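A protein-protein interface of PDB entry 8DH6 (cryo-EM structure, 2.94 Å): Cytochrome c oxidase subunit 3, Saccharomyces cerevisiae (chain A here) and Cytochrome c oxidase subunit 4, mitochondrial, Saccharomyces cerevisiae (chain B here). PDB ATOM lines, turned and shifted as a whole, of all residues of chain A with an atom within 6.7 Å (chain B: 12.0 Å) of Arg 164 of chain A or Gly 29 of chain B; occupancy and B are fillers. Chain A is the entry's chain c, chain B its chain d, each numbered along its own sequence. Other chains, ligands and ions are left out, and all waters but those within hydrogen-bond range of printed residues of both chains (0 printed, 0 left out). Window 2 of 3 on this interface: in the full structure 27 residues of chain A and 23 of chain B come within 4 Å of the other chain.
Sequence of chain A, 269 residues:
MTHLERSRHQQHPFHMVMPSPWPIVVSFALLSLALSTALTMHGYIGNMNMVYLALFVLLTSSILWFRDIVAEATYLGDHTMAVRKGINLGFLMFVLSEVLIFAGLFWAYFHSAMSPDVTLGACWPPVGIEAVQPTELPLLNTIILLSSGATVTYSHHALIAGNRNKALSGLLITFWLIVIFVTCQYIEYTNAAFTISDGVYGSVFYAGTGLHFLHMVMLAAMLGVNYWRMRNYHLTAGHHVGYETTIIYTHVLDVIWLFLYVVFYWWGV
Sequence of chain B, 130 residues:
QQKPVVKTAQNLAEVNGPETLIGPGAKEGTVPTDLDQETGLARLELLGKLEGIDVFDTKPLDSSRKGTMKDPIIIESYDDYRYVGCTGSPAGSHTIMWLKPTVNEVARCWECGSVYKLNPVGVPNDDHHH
Among the printed residues, merely in contact across the chains: Leu 159 of chain A with Val 31 of chain B (3.8 Å), Gly 162 of chain A with Val 31 of chain B (3.4 Å), Arg 164 of chain A with Gly 29 of chain B (3.3 Å), Arg 164 of chain A with Val 31 of chain B (3.6 Å), Tyr 233 of chain A with Gly 29 of chain B (3.3 Å), Tyr 233 of chain A with Thr 30 of chain B (3.2 Å) and Tyr 233 of chain A with Pro 32 of chain B (3.4 Å).
No residue of chain B comes within 4 Å of Asn 163 of chain A.
No residue of chain B comes within 4 Å of Leu 168 of chain A.
Met 230 of chain A touches none of the printed residues of chain B.
No residue of chain B comes within 4 Å of Arg 231 of chain A.
No residue of chain B comes within 4 Å of Asn 232 of chain A.
Of the printed residues of chain B, Tyr 233 of chain A touches Glu 28, Gly 29, Thr 30, Pro 32 and Gln 37.
Of chain A, only Arg 164 (3.3 Å) and Tyr 233 (3.3 Å) come within 4 Å of Gly 29 of chain B.
Printed residues of chain A within 4 Å of Thr 30 of chain B: Tyr 233.
The nearest residue of chain A that does not touch Gly 29 of chain B is Asn 165 of chain A (5.5 Å).
Hydrophobic or aromatic side chains of chain A within 4 Å of the printed part of chain B: Leu 159 and Tyr 233.
Printed residues of chain B that touch a printed residue of chain A: Glu 28, Gly 29, Thr 30, Val 31, Pro 32 and Gln 37.
Hydrophobic or aromatic side chains of chain B within 4 Å of the printed part of chain A: Val 31 and Pro 32.
Among the printed residues, 9 pairs touch across the chains.
The backbone carbonyl oxygen (O) of Tyr 233 of chain A sits close to the side-chain amide oxygen (OE1) of Gln 37 of chain B, 2.9 Å away.
The backbone carbonyl oxygen (O) of Glu 28 of chain B sits close to the side-chain hydroxyl (OH) of Tyr 233 of chain A, 2.3 Å away.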
ATOM      1  N   ALA A 158       5.923  26.421  -2.336  1.00  0.00           N
ATOM      2  CA  ALA A 158       7.005  25.785  -3.079  1.00  0.00           C
ATOM      3  C   ALA A 158       6.956  24.267  -2.959  1.00  0.00           C
ATOM      4  O   ALA A 158       7.290  23.562  -3.916  1.00  0.00           O
ATOM      5  CB  ALA A 158       8.355  26.314  -2.599  1.00  0.00           C
ATOM      6  N   LEU A 159       6.565  23.750  -1.792  1.00  0.00           N
ATOM      7  CA  LEU A 159       6.392  22.310  -1.638  1.00  0.00           C
ATOM      8  C   LEU A 159       5.275  21.792  -2.529  1.00  0.00           C
ATOM      9  O   LEU A 159       5.422  20.747  -3.174  1.00  0.00           O
ATOM     10  CB  LEU A 159       6.103  21.964  -0.178  1.00  0.00           C
ATOM     11  CG  LEU A 159       5.777  20.501   0.124  1.00  0.00           C
ATOM     12  CD1 LEU A 159       6.969  19.609  -0.176  1.00  0.00           C
ATOM     13  CD2 LEU A 159       5.325  20.333   1.563  1.00  0.00           C
ATOM     14  N   GLY A 162       6.301  21.562  -6.115  1.00  0.00           N
ATOM     15  CA  GLY A 162       7.205  20.473  -6.411  1.00  0.00           C
ATOM     16  C   GLY A 162       8.677  20.804  -6.296  1.00  0.00           C
ATOM     17  O   GLY A 162       9.510  19.951  -6.625  1.00  0.00           O
ATOM     18  N   ASN A 163       9.025  22.006  -5.846  1.00  0.00           N
ATOM     19  CA  ASN A 163      10.423  22.404  -5.722  1.00  0.00           C
ATOM     20  C   ASN A 163      10.890  22.126  -4.299  1.00  0.00           C
ATOM     21  O   ASN A 163      10.414  22.751  -3.348  1.00  0.00           O
ATOM     22  CB  ASN A 163      10.585  23.875  -6.089  1.00  0.00           C
ATOM     23  CG  ASN A 163      12.033  24.277  -6.257  1.00  0.00           C
ATOM     24  OD1 ASN A 163      12.938  23.452  -6.143  1.00  0.00           O
ATOM     25  ND2 ASN A 163      12.260  25.551  -6.546  1.00  0.00           N
ATOM     26  N   ARG A 164      11.825  21.185  -4.150  1.00  0.00           N
ATOM     27  CA  ARG A 164      12.255  20.767  -2.820  1.00  0.00           C
ATOM     28  C   ARG A 164      13.159  21.807  -2.169  1.00  0.00           C
ATOM     29  O   ARG A 164      13.034  22.088  -0.969  1.00  0.00           O
ATOM     30  CB  ARG A 164      12.970  19.419  -2.902  1.00  0.00           C
ATOM     31  CG  ARG A 164      13.431  18.885  -1.564  1.00  0.00           C
ATOM     32  CD  ARG A 164      14.165  17.573  -1.722  1.00  0.00           C
ATOM     33  NE  ARG A 164      14.351  16.895  -0.445  1.00  0.00           N
ATOM     34  CZ  ARG A 164      15.515  16.793   0.181  1.00  0.00           C
ATOM     35  NH1 ARG A 164      16.619  17.321  -0.321  1.00  0.00           N
ATOM     36  NH2 ARG A 164      15.572  16.146   1.340  1.00  0.00           N
ATOM     37  N   ASN A 165      14.087  22.377  -2.941  1.00  0.00           N
ATOM     38  CA  ASN A 165      15.097  23.256  -2.362  1.00  0.00           C
ATOM     39  C   ASN A 165      14.482  24.510  -1.756  1.00  0.00           C
ATOM     40  O   ASN A 165      14.840  24.896  -0.637  1.00  0.00           O
ATOM     41  CB  ASN A 165      16.129  23.634  -3.423  1.00  0.00           C
ATOM     42  CG  ASN A 165      16.977  22.455  -3.853  1.00  0.00           C
ATOM     43  OD1 ASN A 165      17.065  22.140  -5.040  1.00  0.00           O
ATOM     44  ND2 ASN A 165      17.596  21.789  -2.887  1.00  0.00           N
ATOM     45  N   LYS A 166      13.558  25.154  -2.472  1.00  0.00           N
ATOM     46  CA  LYS A 166      12.925  26.359  -1.947  1.00  0.00           C
ATOM     47  C   LYS A 166      12.099  26.051  -0.707  1.00  0.00           C
ATOM     48  O   LYS A 166      12.107  26.826   0.257  1.00  0.00           O
ATOM     49  CB  LYS A 166      12.062  27.012  -3.023  1.00  0.00           C
ATOM     50  CG  LYS A 166      12.859  27.624  -4.160  1.00  0.00           C
ATOM     51  CD  LYS A 166      13.896  28.608  -3.644  1.00  0.00           C
ATOM     52  CE  LYS A 166      14.707  29.203  -4.784  1.00  0.00           C
ATOM     53  NZ  LYS A 166      15.799  30.084  -4.287  1.00  0.00           N
ATOM     54  N   ALA A 167      11.379  24.928  -0.712  1.00  0.00           N
ATOM     55  CA  ALA A 167      10.582  24.554   0.451  1.00  0.00           C
ATOM     56  C   ALA A 167      11.465  24.326   1.670  1.00  0.00           C
ATOM     57  O   ALA A 167      11.173  24.828   2.766  1.00  0.00           O
ATOM     58  CB  ALA A 167       9.757  23.306   0.143  1.00  0.00           C
ATOM     59  N   LEU A 168      12.559  23.580   1.497  1.00  0.00           N
ATOM     60  CA  LEU A 168      13.466  23.332   2.613  1.00  0.00           C
ATOM     61  C   LEU A 168      14.091  24.625   3.116  1.00  0.00           C
ATOM     62  O   LEU A 168      14.185  24.841   4.330  1.00  0.00           O
ATOM     63  CB  LEU A 168      14.555  22.343   2.201  1.00  0.00           C
ATOM     64  CG  LEU A 168      14.148  20.879   2.081  1.00  0.00           C
ATOM     65  CD1 LEU A 168      15.265  20.092   1.431  1.00  0.00           C
ATOM     66  CD2 LEU A 168      13.808  20.307   3.440  1.00  0.00           C
ATOM     67  N   SER A 169      14.525  25.497   2.201  1.00  0.00           N
ATOM     68  CA  SER A 169      15.139  26.754   2.613  1.00  0.00           C
ATOM     69  C   SER A 169      14.155  27.624   3.382  1.00  0.00           C
ATOM     70  O   SER A 169      14.502  28.184   4.431  1.00  0.00           O
ATOM     71  CB  SER A 169      15.672  27.498   1.391  1.00  0.00           C
ATOM     72  OG  SER A 169      16.214  28.755   1.752  1.00  0.00           O
ATOM     73  N   MET A 230      10.263  16.509   5.921  1.00  0.00           N
ATOM     74  CA  MET A 230      10.408  16.959   4.542  1.00  0.00           C
ATOM     75  C   MET A 230      11.786  16.641   3.982  1.00  0.00           C
ATOM     76  O   MET A 230      11.910  16.327   2.794  1.00  0.00           O
ATOM     77  CB  MET A 230      10.140  18.463   4.452  1.00  0.00           C
ATOM     78  CG  MET A 230      10.353  19.056   3.070  1.00  0.00           C
ATOM     79  SD  MET A 230       9.799  20.765   2.918  1.00  0.00           S
ATOM     80  CE  MET A 230       8.509  20.826   4.155  1.00  0.00           C
ATOM     81  N   ARG A 231      12.825  16.720   4.814  1.00  0.00           N
ATOM     82  CA  ARG A 231      14.172  16.415   4.351  1.00  0.00           C
ATOM     83  C   ARG A 231      14.298  14.956   3.934  1.00  0.00           C
ATOM     84  O   ARG A 231      14.938  14.649   2.922  1.00  0.00           O
ATOM     85  CB  ARG A 231      15.185  16.752   5.444  1.00  0.00           C
ATOM     86  CG  ARG A 231      16.567  17.087   4.931  1.00  0.00           C
ATOM     87  CD  ARG A 231      17.538  17.257   6.080  1.00  0.00           C
ATOM     88  NE  ARG A 231      18.174  15.995   6.434  1.00  0.00           N
ATOM     89  CZ  ARG A 231      19.389  15.635   6.047  1.00  0.00           C
ATOM     90  NH1 ARG A 231      20.136  16.426   5.294  1.00  0.00           N
ATOM     91  NH2 ARG A 231      19.866  14.454   6.424  1.00  0.00           N
ATOM     92  N   ASN A 232      13.693  14.043   4.694  1.00  0.00           N
ATOM     93  CA  ASN A 232      13.780  12.613   4.426  1.00  0.00           C
ATOM     94  C   ASN A 232      12.588  12.095   3.630  1.00  0.00           C
ATOM     95  O   ASN A 232      12.212  10.927   3.764  1.00  0.00           O
ATOM     96  CB  ASN A 232      13.927  11.839   5.733  1.00  0.00           C
ATOM     97  CG  ASN A 232      15.143  12.264   6.520  1.00  0.00           C
ATOM     98  OD1 ASN A 232      15.085  12.418   7.736  1.00  0.00           O
ATOM     99  ND2 ASN A 232      16.256  12.462   5.827  1.00  0.00           N
ATOM    100  N   TYR A 233      11.980  12.956   2.813  1.00  0.00           N
ATOM    101  CA  TYR A 233      10.972  12.560   1.831  1.00  0.00           C
ATOM    102  C   TYR A 233       9.726  11.963   2.479  1.00  0.00           C
ATOM    103  O   TYR A 233       9.021  11.162   1.864  1.00  0.00           O
ATOM    104  CB  TYR A 233      11.559  11.583   0.809  1.00  0.00           C
ATOM    105  CG  TYR A 233      12.798  12.100   0.114  1.00  0.00           C
ATOM    106  CD1 TYR A 233      12.703  12.842  -1.054  1.00  0.00           C
ATOM    107  CD2 TYR A 233      14.059  11.846   0.627  1.00  0.00           C
ATOM    108  CE1 TYR A 233      13.829  13.313  -1.691  1.00  0.00           C
ATOM    109  CE2 TYR A 233      15.191  12.314  -0.003  1.00  0.00           C
ATOM    110  CZ  TYR A 233      15.070  13.046  -1.160  1.00  0.00           C
ATOM    111  OH  TYR A 233      16.201  13.512  -1.789  1.00  0.00           O
ATOM    112  N   PRO B  24       7.362   2.808  -6.067  1.00  0.00           N
ATOM    113  CA  PRO B  24       8.701   3.385  -5.912  1.00  0.00           C
ATOM    114  C   PRO B  24       8.661   4.837  -5.460  1.00  0.00           C
ATOM    115  O   PRO B  24       7.783   5.615  -5.842  1.00  0.00           O
ATOM    116  CB  PRO B  24       9.278   3.269  -7.327  1.00  0.00           C
ATOM    117  CG  PRO B  24       8.077   3.436  -8.215  1.00  0.00           C
ATOM    118  CD  PRO B  24       6.858   2.965  -7.442  1.00  0.00           C
ATOM    119  N   GLY B  25       9.642   5.210  -4.647  1.00  0.00           N
ATOM    120  CA  GLY B  25       9.690   6.540  -4.080  1.00  0.00           C
ATOM    121  C   GLY B  25      10.295   7.565  -5.023  1.00  0.00           C
ATOM    122  O   GLY B  25      10.501   7.333  -6.215  1.00  0.00           O
ATOM    123  N   ALA B  26      10.576   8.739  -4.462  1.00  0.00           N
ATOM    124  CA  ALA B  26      11.237   9.796  -5.213  1.00  0.00           C
ATOM    125  C   ALA B  26      12.647   9.363  -5.596  1.00  0.00           C
ATOM    126  O   ALA B  26      13.240   8.483  -4.966  1.00  0.00           O
ATOM    127  CB  ALA B  26      11.284  11.087  -4.398  1.00  0.00           C
ATOM    128  N   LYS B  27      13.189   9.989  -6.641  1.00  0.00           N
ATOM    129  CA  LYS B  27      14.398   9.441  -7.256  1.00  0.00           C
ATOM    130  C   LYS B  27      15.651   9.770  -6.448  1.00  0.00           C
ATOM    131  O   LYS B  27      16.267   8.880  -5.851  1.00  0.00           O
ATOM    132  CB  LYS B  27      14.527   9.957  -8.693  1.00  0.00           C
ATOM    133  CG  LYS B  27      13.347   9.606  -9.586  1.00  0.00           C
ATOM    134  CD  LYS B  27      13.656   9.894 -11.046  1.00  0.00           C
ATOM    135  CE  LYS B  27      14.788   9.016 -11.555  1.00  0.00           C
ATOM    136  NZ  LYS B  27      15.242   9.426 -12.912  1.00  0.00           N
ATOM    137  N   GLU B  28      16.048  11.042  -6.413  1.00  0.00           N
ATOM    138  CA  GLU B  28      17.192  11.408  -5.585  1.00  0.00           C
ATOM    139  C   GLU B  28      16.961  12.669  -4.763  1.00  0.00           C
ATOM    140  O   GLU B  28      17.335  12.725  -3.587  1.00  0.00           O
ATOM    141  CB  GLU B  28      18.437  11.584  -6.459  1.00  0.00           C
ATOM    142  CG  GLU B  28      19.729  11.707  -5.670  1.00  0.00           C
ATOM    143  CD  GLU B  28      19.796  10.733  -4.510  1.00  0.00           C
ATOM    144  OE1 GLU B  28      19.870   9.511  -4.760  1.00  0.00           O
ATOM    145  OE2 GLU B  28      19.774  11.189  -3.347  1.00  0.00           O
ATOM    146  N   GLY B  29      16.344  13.683  -5.367  1.00  0.00           N
ATOM    147  CA  GLY B  29      16.281  14.989  -4.742  1.00  0.00           C
ATOM    148  C   GLY B  29      15.023  15.781  -5.024  1.00  0.00           C
ATOM    149  O   GLY B  29      14.998  16.999  -4.824  1.00  0.00           O
ATOM    150  N   THR B  30      13.980  15.115  -5.500  1.00  0.00           N
ATOM    151  CA  THR B  30      12.701  15.754  -5.763  1.00  0.00           C
ATOM    152  C   THR B  30      11.695  15.371  -4.686  1.00  0.00           C
ATOM    153  O   THR B  30      11.826  14.341  -4.021  1.00  0.00           O
ATOM    154  CB  THR B  30      12.168  15.357  -7.140  1.00  0.00           C
ATOM    155  OG1 THR B  30      12.254  13.936  -7.292  1.00  0.00           O
ATOM    156  CG2 THR B  30      12.977  16.029  -8.238  1.00  0.00           C
ATOM    157  N   VAL B  31      10.687  16.219  -4.516  1.00  0.00           N
ATOM    158  CA  VAL B  31       9.644  15.956  -3.529  1.00  0.00           C
ATOM    159  C   VAL B  31       8.862  14.721  -3.960  1.00  0.00           C
ATOM    160  O   VAL B  31       8.599  14.537  -5.157  1.00  0.00           O
ATOM    161  CB  VAL B  31       8.718  17.170  -3.344  1.00  0.00           C
ATOM    162  CG1 VAL B  31       9.496  18.347  -2.784  1.00  0.00           C
ATOM    163  CG2 VAL B  31       8.066  17.545  -4.653  1.00  0.00           C
ATOM    164  N   PRO B  32       8.508  13.833  -3.035  1.00  0.00           N
ATOM    165  CA  PRO B  32       7.686  12.680  -3.406  1.00  0.00           C
ATOM    166  C   PRO B  32       6.307  13.118  -3.865  1.00  0.00           C
ATOM    167  O   PRO B  32       5.755  14.107  -3.380  1.00  0.00           O
ATOM    168  CB  PRO B  32       7.611  11.863  -2.110  1.00  0.00           C
ATOM    169  CG  PRO B  32       8.745  12.354  -1.280  1.00  0.00           C
ATOM    170  CD  PRO B  32       8.898  13.796  -1.619  1.00  0.00           C
ATOM    171  N   THR B  33       5.755  12.376  -4.818  1.00  0.00           N
ATOM    172  CA  THR B  33       4.392  12.623  -5.251  1.00  0.00           C
ATOM    173  C   THR B  33       3.443  11.637  -4.576  1.00  0.00           C
ATOM    174  O   THR B  33       3.856  10.715  -3.871  1.00  0.00           O
ATOM    175  CB  THR B  33       4.280  12.520  -6.770  1.00  0.00           C
ATOM    176  OG1 THR B  33       4.707  11.222  -7.195  1.00  0.00           O
ATOM    177  CG2 THR B  33       5.152  13.568  -7.432  1.00  0.00           C
ATOM    178  N   ASP B  36       3.923   8.159  -5.812  1.00  0.00           N
ATOM    179  CA  ASP B  36       5.223   7.560  -5.527  1.00  0.00           C
ATOM    180  C   ASP B  36       5.211   6.764  -4.227  1.00  0.00           C
ATOM    181  O   ASP B  36       5.562   5.580  -4.210  1.00  0.00           O
ATOM    182  CB  ASP B  36       6.302   8.645  -5.477  1.00  0.00           C
ATOM    183  CG  ASP B  36       6.879   8.961  -6.842  1.00  0.00           C
ATOM    184  OD1 ASP B  36       7.656   8.136  -7.365  1.00  0.00           O
ATOM    185  OD2 ASP B  36       6.565  10.036  -7.391  1.00  0.00           O
ATOM    186  N   GLN B  37       4.807   7.393  -3.123  1.00  0.00           N
ATOM    187  CA  GLN B  37       5.033   6.817  -1.804  1.00  0.00           C
ATOM    188  C   GLN B  37       3.761   6.570  -1.003  1.00  0.00           C
ATOM    189  O   GLN B  37       3.851   6.154   0.157  1.00  0.00           O
ATOM    190  CB  GLN B  37       5.984   7.712  -1.006  1.00  0.00           C
ATOM    191  CG  GLN B  37       7.371   7.790  -1.607  1.00  0.00           C
ATOM    192  CD  GLN B  37       8.377   8.401  -0.665  1.00  0.00           C
ATOM    193  OE1 GLN B  37       8.027   8.861   0.418  1.00  0.00           O
ATOM    194  NE2 GLN B  37       9.639   8.409  -1.074  1.00  0.00           N
